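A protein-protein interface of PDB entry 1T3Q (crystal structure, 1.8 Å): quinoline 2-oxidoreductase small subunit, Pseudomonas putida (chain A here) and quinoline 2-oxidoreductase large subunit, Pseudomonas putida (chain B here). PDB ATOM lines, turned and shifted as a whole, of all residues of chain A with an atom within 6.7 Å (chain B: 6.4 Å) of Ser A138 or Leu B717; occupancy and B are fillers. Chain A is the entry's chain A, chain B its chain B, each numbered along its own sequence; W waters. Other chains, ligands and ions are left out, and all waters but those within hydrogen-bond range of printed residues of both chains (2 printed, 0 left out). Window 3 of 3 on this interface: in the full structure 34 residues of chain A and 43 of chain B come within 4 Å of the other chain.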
ATOM      1  N   VAL A  52     -17.040  28.597  -5.830  1.00  0.00           N
ATOM      2  CA  VAL A  52     -16.925  27.204  -5.417  1.00  0.00           C
ATOM      3  C   VAL A  52     -17.058  26.869  -3.927  1.00  0.00           C
ATOM      4  O   VAL A  52     -17.805  25.958  -3.563  1.00  0.00           O
ATOM      5  CB  VAL A  52     -15.580  26.589  -5.908  1.00  0.00           C
ATOM      6  CG1 VAL A  52     -15.493  25.122  -5.489  1.00  0.00           C
ATOM      7  CG2 VAL A  52     -15.462  26.715  -7.428  1.00  0.00           C
ATOM      8  N   ARG A  66     -24.110  33.360  -4.212  1.00  0.00           N
ATOM      9  CA  ARG A  66     -22.700  33.626  -3.934  1.00  0.00           C
ATOM     10  C   ARG A  66     -22.509  35.134  -4.034  1.00  0.00           C
ATOM     11  O   ARG A  66     -22.675  35.709  -5.113  1.00  0.00           O
ATOM     12  CB  ARG A  66     -21.803  32.938  -4.971  1.00  0.00           C
ATOM     13  CG  ARG A  66     -21.958  31.434  -5.072  1.00  0.00           C
ATOM     14  CD  ARG A  66     -21.654  30.716  -3.759  1.00  0.00           C
ATOM     15  NE  ARG A  66     -21.240  29.342  -4.022  1.00  0.00           N
ATOM     16  CZ  ARG A  66     -21.645  28.271  -3.347  1.00  0.00           C
ATOM     17  NH1 ARG A  66     -21.193  27.073  -3.693  1.00  0.00           N
ATOM     18  NH2 ARG A  66     -22.504  28.386  -2.340  1.00  0.00           N
ATOM     19  N   THR A 117     -27.176  28.432   3.634  1.00  0.00           N
ATOM     20  CA  THR A 117     -27.711  27.300   2.893  1.00  0.00           C
ATOM     21  C   THR A 117     -28.665  26.485   3.769  1.00  0.00           C
ATOM     22  O   THR A 117     -29.733  26.075   3.313  1.00  0.00           O
ATOM     23  CB  THR A 117     -26.584  26.385   2.367  1.00  0.00           C
ATOM     24  OG1 THR A 117     -25.724  27.139   1.502  1.00  0.00           O
ATOM     25  CG2 THR A 117     -27.169  25.219   1.574  1.00  0.00           C
ATOM     26  N   ASP A 131     -29.632  12.550   3.991  1.00  0.00           N
ATOM     27  CA  ASP A 131     -29.208  12.512   2.592  1.00  0.00           C
ATOM     28  C   ASP A 131     -29.564  13.793   1.856  1.00  0.00           C
ATOM     29  O   ASP A 131     -28.779  14.288   1.051  1.00  0.00           O
ATOM     30  CB  ASP A 131     -29.839  11.320   1.867  1.00  0.00           C
ATOM     31  CG  ASP A 131     -29.063  10.038   2.079  1.00  0.00           C
ATOM     32  OD1 ASP A 131     -29.585   8.959   1.733  1.00  0.00           O
ATOM     33  OD2 ASP A 131     -27.922  10.112   2.578  1.00  0.00           O
ATOM     34  N   VAL A 133     -29.945  16.734   3.209  1.00  0.00           N
ATOM     35  CA  VAL A 133     -29.084  17.794   3.713  1.00  0.00           C
ATOM     36  C   VAL A 133     -27.697  17.694   3.076  1.00  0.00           C
ATOM     37  O   VAL A 133     -27.157  18.693   2.605  1.00  0.00           O
ATOM     38  CB  VAL A 133     -28.957  17.742   5.252  1.00  0.00           C
ATOM     39  CG1 VAL A 133     -28.010  18.839   5.734  1.00  0.00           C
ATOM     40  CG2 VAL A 133     -30.334  17.940   5.894  1.00  0.00           C
ATOM     41  N   ARG A 134     -27.126  16.495   3.044  1.00  0.00           N
ATOM     42  CA  ARG A 134     -25.805  16.329   2.444  1.00  0.00           C
ATOM     43  C   ARG A 134     -25.819  16.770   0.981  1.00  0.00           C
ATOM     44  O   ARG A 134     -24.853  17.356   0.493  1.00  0.00           O
ATOM     45  CB  ARG A 134     -25.334  14.874   2.560  1.00  0.00           C
ATOM     46  CG  ARG A 134     -24.823  14.504   3.960  1.00  0.00           C
ATOM     47  CD  ARG A 134     -24.408  13.038   4.042  1.00  0.00           C
ATOM     48  NE  ARG A 134     -23.912  12.653   5.365  1.00  0.00           N
ATOM     49  CZ  ARG A 134     -22.689  12.918   5.820  1.00  0.00           C
ATOM     50  NH1 ARG A 134     -21.822  13.575   5.063  1.00  0.00           N
ATOM     51  NH2 ARG A 134     -22.329  12.515   7.030  1.00  0.00           N
ATOM     52  N   GLU A 135     -26.927  16.502   0.294  1.00  0.00           N
ATOM     53  CA  GLU A 135     -27.076  16.872  -1.108  1.00  0.00           C
ATOM     54  C   GLU A 135     -27.101  18.377  -1.310  1.00  0.00           C
ATOM     55  O   GLU A 135     -26.369  18.915  -2.141  1.00  0.00           O
ATOM     56  CB  GLU A 135     -28.363  16.266  -1.675  1.00  0.00           C
ATOM     57  CG  GLU A 135     -28.338  14.754  -1.739  1.00  0.00           C
ATOM     58  CD  GLU A 135     -29.699  14.145  -2.024  1.00  0.00           C
ATOM     59  OE1 GLU A 135     -29.774  12.900  -2.129  1.00  0.00           O
ATOM     60  OE2 GLU A 135     -30.691  14.902  -2.135  1.00  0.00           O
ATOM     61  N   VAL A 136     -27.946  19.065  -0.554  1.00  0.00           N
ATOM     62  CA  VAL A 136     -28.048  20.510  -0.691  1.00  0.00           C
ATOM     63  C   VAL A 136     -26.831  21.245  -0.131  1.00  0.00           C
ATOM     64  O   VAL A 136     -26.451  22.298  -0.641  1.00  0.00           O
ATOM     65  CB  VAL A 136     -29.324  21.037  -0.010  1.00  0.00           C
ATOM     66  CG1 VAL A 136     -29.481  22.531  -0.279  1.00  0.00           C
ATOM     67  CG2 VAL A 136     -30.536  20.280  -0.546  1.00  0.00           C
ATOM     68  N   MET A 137     -26.207  20.685   0.904  1.00  0.00           N
ATOM     69  CA  MET A 137     -25.039  21.323   1.512  1.00  0.00           C
ATOM     70  C   MET A 137     -23.746  21.014   0.751  1.00  0.00           C
ATOM     71  O   MET A 137     -22.684  21.525   1.105  1.00  0.00           O
ATOM     72  CB  MET A 137     -24.880  20.867   2.970  1.00  0.00           C
ATOM     73  CG  MET A 137     -26.052  21.193   3.909  1.00  0.00           C
ATOM     74  SD  MET A 137     -26.411  22.954   4.095  1.00  0.00           S
ATOM     75  CE  MET A 137     -24.864  23.559   4.846  1.00  0.00           C
ATOM     76  N   SER A 138     -23.834  20.203  -0.301  1.00  0.00           N
ATOM     77  CA  SER A 138     -22.647  19.817  -1.069  1.00  0.00           C
ATOM     78  C   SER A 138     -21.924  20.978  -1.745  1.00  0.00           C
ATOM     79  O   SER A 138     -20.822  20.806  -2.270  1.00  0.00           O
ATOM     80  CB  SER A 138     -23.001  18.751  -2.119  1.00  0.00           C
ATOM     81  OG  SER A 138     -23.808  19.271  -3.157  1.00  0.00           O
ATOM     82  N   GLY A 139     -22.544  22.154  -1.732  1.00  0.00           N
ATOM     83  CA  GLY A 139     -21.937  23.326  -2.334  1.00  0.00           C
ATOM     84  C   GLY A 139     -21.249  24.220  -1.315  1.00  0.00           C
ATOM     85  O   GLY A 139     -20.807  25.323  -1.642  1.00  0.00           O
ATOM     86  N   ASN A 140     -21.170  23.757  -0.069  1.00  0.00           N
ATOM     87  CA  ASN A 140     -20.511  24.517   0.990  1.00  0.00           C
ATOM     88  C   ASN A 140     -19.337  23.696   1.515  1.00  0.00           C
ATOM     89  O   ASN A 140     -19.522  22.615   2.074  1.00  0.00           O
ATOM     90  CB  ASN A 140     -21.482  24.823   2.134  1.00  0.00           C
ATOM     91  CG  ASN A 140     -22.490  25.903   1.774  1.00  0.00           C
ATOM     92  OD1 ASN A 140     -23.514  25.632   1.145  1.00  0.00           O
ATOM     93  ND2 ASN A 140     -22.196  27.135   2.166  1.00  0.00           N
ATOM     94  N   LEU A 141     -18.129  24.215   1.332  1.00  0.00           N
ATOM     95  CA  LEU A 141     -16.936  23.505   1.765  1.00  0.00           C
ATOM     96  C   LEU A 141     -16.482  23.821   3.181  1.00  0.00           C
ATOM     97  O   LEU A 141     -16.507  24.972   3.621  1.00  0.00           O
ATOM     98  CB  LEU A 141     -15.785  23.790   0.794  1.00  0.00           C
ATOM     99  CG  LEU A 141     -16.101  23.512  -0.680  1.00  0.00           C
ATOM    100  CD1 LEU A 141     -14.914  23.913  -1.552  1.00  0.00           C
ATOM    101  CD2 LEU A 141     -16.437  22.051  -0.862  1.00  0.00           C
ATOM    102  N   TYR A 147     -17.869  17.354   8.163  1.00  0.00           N
ATOM    103  CA  TYR A 147     -19.305  17.488   7.866  1.00  0.00           C
ATOM    104  C   TYR A 147     -20.367  16.768   8.688  1.00  0.00           C
ATOM    105  O   TYR A 147     -21.490  17.266   8.788  1.00  0.00           O
ATOM    106  CB  TYR A 147     -19.569  17.118   6.409  1.00  0.00           C
ATOM    107  CG  TYR A 147     -18.794  17.925   5.400  1.00  0.00           C
ATOM    108  CD1 TYR A 147     -19.099  19.262   5.164  1.00  0.00           C
ATOM    109  CD2 TYR A 147     -17.762  17.343   4.671  1.00  0.00           C
ATOM    110  CE1 TYR A 147     -18.393  20.005   4.213  1.00  0.00           C
ATOM    111  CE2 TYR A 147     -17.051  18.072   3.721  1.00  0.00           C
ATOM    112  CZ  TYR A 147     -17.372  19.397   3.497  1.00  0.00           C
ATOM    113  OH  TYR A 147     -16.685  20.103   2.539  1.00  0.00           O
ATOM    114  N   ARG B 656     -16.316   5.308  -3.694  1.00  0.00           N
ATOM    115  CA  ARG B 656     -17.061   5.877  -2.586  1.00  0.00           C
ATOM    116  C   ARG B 656     -16.620   5.255  -1.264  1.00  0.00           C
ATOM    117  O   ARG B 656     -16.515   4.035  -1.151  1.00  0.00           O
ATOM    118  CB  ARG B 656     -18.560   5.628  -2.828  1.00  0.00           C
ATOM    119  CG  ARG B 656     -19.501   6.117  -1.742  1.00  0.00           C
ATOM    120  CD  ARG B 656     -20.945   6.184  -2.255  1.00  0.00           C
ATOM    121  NE  ARG B 656     -21.855   5.309  -1.515  1.00  0.00           N
ATOM    122  CZ  ARG B 656     -22.157   4.064  -1.870  1.00  0.00           C
ATOM    123  NH1 ARG B 656     -22.993   3.346  -1.130  1.00  0.00           N
ATOM    124  NH2 ARG B 656     -21.638   3.539  -2.969  1.00  0.00           N
ATOM    125  N   PRO B 714     -12.820  17.312  -0.329  1.00  0.00           N
ATOM    126  CA  PRO B 714     -14.083  16.660   0.015  1.00  0.00           C
ATOM    127  C   PRO B 714     -15.280  17.528   0.382  1.00  0.00           C
ATOM    128  O   PRO B 714     -15.158  18.580   1.012  1.00  0.00           O
ATOM    129  CB  PRO B 714     -13.688  15.682   1.129  1.00  0.00           C
ATOM    130  CG  PRO B 714     -12.364  16.183   1.630  1.00  0.00           C
ATOM    131  CD  PRO B 714     -11.690  16.726   0.408  1.00  0.00           C
ATOM    132  N   THR B 715     -16.447  17.054  -0.040  1.00  0.00           N
ATOM    133  CA  THR B 715     -17.712  17.721   0.226  1.00  0.00           C
ATOM    134  C   THR B 715     -18.540  16.781   1.105  1.00  0.00           C
ATOM    135  O   THR B 715     -18.094  15.686   1.453  1.00  0.00           O
ATOM    136  CB  THR B 715     -18.500  17.952  -1.065  1.00  0.00           C
ATOM    137  OG1 THR B 715     -18.902  16.682  -1.596  1.00  0.00           O
ATOM    138  CG2 THR B 715     -17.648  18.672  -2.103  1.00  0.00           C
ATOM    139  N   THR B 716     -19.745  17.216   1.455  1.00  0.00           N
ATOM    140  CA  THR B 716     -20.656  16.415   2.267  1.00  0.00           C
ATOM    141  C   THR B 716     -20.967  15.074   1.594  1.00  0.00           C
ATOM    142  O   THR B 716     -21.418  14.133   2.249  1.00  0.00           O
ATOM    143  CB  THR B 716     -21.992  17.152   2.463  1.00  0.00           C
ATOM    144  OG1 THR B 716     -22.437  17.640   1.193  1.00  0.00           O
ATOM    145  CG2 THR B 716     -21.844  18.311   3.430  1.00  0.00           C
ATOM    146  N   LEU B 717     -20.724  14.987   0.291  1.00  0.00           N
ATOM    147  CA  LEU B 717     -21.011  13.765  -0.455  1.00  0.00           C
ATOM    148  C   LEU B 717     -19.825  12.808  -0.555  1.00  0.00           C
ATOM    149  O   LEU B 717     -19.951  11.707  -1.096  1.00  0.00           O
ATOM    150  CB  LEU B 717     -21.502  14.122  -1.862  1.00  0.00           C
ATOM    151  CG  LEU B 717     -22.773  14.988  -1.901  1.00  0.00           C
ATOM    152  CD1 LEU B 717     -23.077  15.414  -3.330  1.00  0.00           C
ATOM    153  CD2 LEU B 717     -23.934  14.210  -1.312  1.00  0.00           C
ATOM    154  N   ASP B 718     -18.682  13.229  -0.033  1.00  0.00           N
ATOM    155  CA  ASP B 718     -17.470  12.416  -0.070  1.00  0.00           C
ATOM    156  C   ASP B 718     -17.151  11.751   1.253  1.00  0.00           C
ATOM    157  O   ASP B 718     -16.483  10.718   1.284  1.00  0.00           O
ATOM    158  CB  ASP B 718     -16.272  13.275  -0.474  1.00  0.00           C
ATOM    159  CG  ASP B 718     -16.393  13.819  -1.876  1.00  0.00           C
ATOM    160  OD1 ASP B 718     -16.462  13.006  -2.820  1.00  0.00           O
ATOM    161  OD2 ASP B 718     -16.419  15.055  -2.033  1.00  0.00           O
ATOM    162  N   VAL B 719     -17.620  12.342   2.348  1.00  0.00           N
ATOM    163  CA  VAL B 719     -17.339  11.810   3.674  1.00  0.00           C
ATOM    164  C   VAL B 719     -18.567  11.138   4.270  1.00  0.00           C
ATOM    165  O   VAL B 719     -19.633  11.749   4.380  1.00  0.00           O
ATOM    166  CB  VAL B 719     -16.865  12.935   4.626  1.00  0.00           C
ATOM    167  CG1 VAL B 719     -16.255  12.335   5.891  1.00  0.00           C
ATOM    168  CG2 VAL B 719     -15.856  13.829   3.911  1.00  0.00           C
ATOM    169  N   PRO B 720     -18.431   9.864   4.669  1.00  0.00           N
ATOM    170  CA  PRO B 720     -19.549   9.121   5.257  1.00  0.00           C
ATOM    171  C   PRO B 720     -19.676   9.452   6.732  1.00  0.00           C
ATOM    172  O   PRO B 720     -18.879  10.221   7.276  1.00  0.00           O
ATOM    173  CB  PRO B 720     -19.127   7.675   5.054  1.00  0.00           C
ATOM    174  CG  PRO B 720     -17.637   7.760   5.345  1.00  0.00           C
ATOM    175  CD  PRO B 720     -17.226   9.014   4.577  1.00  0.00           C
HETATM  176  O   HOH W   1     -19.474  13.106   7.302  1.00  0.00           O
HETATM  177  O   HOH W   2     -19.880  20.104   1.090  1.00  0.00           O
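The backbone carbonyl oxygen (O) of Arg A134 lies within hydrogen-bond range of the side-chain hydroxyl (OG1) of Thr B716. The backbone carbonyl oxygen of Val B719 sits at hydrogen-bond distance from the guanidinium group of Arg A134, at 2.9 Å. The side-chain hydroxyl (OG1) of Thr B716 sits close to the backbone NH (N) of Ser A138. The side-chain hydroxyl (OH) of Tyr A147 sits at hydrogen-bond distance from the backbone carbonyl oxygen (O) of Pro B714 (2.6 Å).
Water W2 lies within hydrogen-bond range of O of Asn A140, N of Thr B716 and O of Met A137. Water W1 lies within hydrogen-bond range of the guanidinium group of Arg A134, the backbone carbonyl oxygen of Pro B720 and the backbone carbonyl oxygen of Val B719.
Val A133 touches none of the printed residues of chain B. Printed residues of chain B within 4 Å of Arg A134: Thr B716, Leu B717 and Val B719. Of the printed residues of chain B, Met A137 touches Thr B716 (3.6 Å). Of the printed residues of chain B, Ser A138 touches Thr B715 (3.8 Å), Thr B716 (3.1 Å) and Leu B717 (3.6 Å). Printed residues of chain B within 4 Å of Leu A141: Thr B715. Of the printed residues of chain A, Pro B714 touches Tyr A147. Of chain A, only Arg A134 (3.7 Å) and Ser A138 (3.6 Å) come within 4 Å of Leu B717. Printed residues of chain A within 4 Å of Val B719: Arg A134 (2.9 Å). The nearest printed residue of chain B that does not touch Tyr A147 is Val B719 (4.1 Å).
Of the 14 printed residues of chain A, 5 touch a printed residue of chain B. Hydrophobic or aromatic side chains of chain A within 4 Å of the printed part of chain B: Met A137, Leu A141 and Tyr A147.
Leu B717 touches Arg A134. Met A137 touches Thr B716. Ser A138 touches Thr B715. Leu B717 touches Ser A138 (CD1 to CB, 3.6 Å). Leu A141 touches Thr B715. Tyr A147 touches Thr B715. Thr B716 touches Tyr A147 (CG2 to CD1, 3.4 Å).
O of Glu A135 sits at hydrogen-bond distance from OG of Ser A138. The backbone NH (N) of Leu B717 sits close to the side-chain hydroxyl (OG1) of Thr B715, at 3.1 Å. The backbone NH of Thr B715 sits at hydrogen-bond distance from the side-chain carboxylate of Asp B718, at 2.8 Å.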
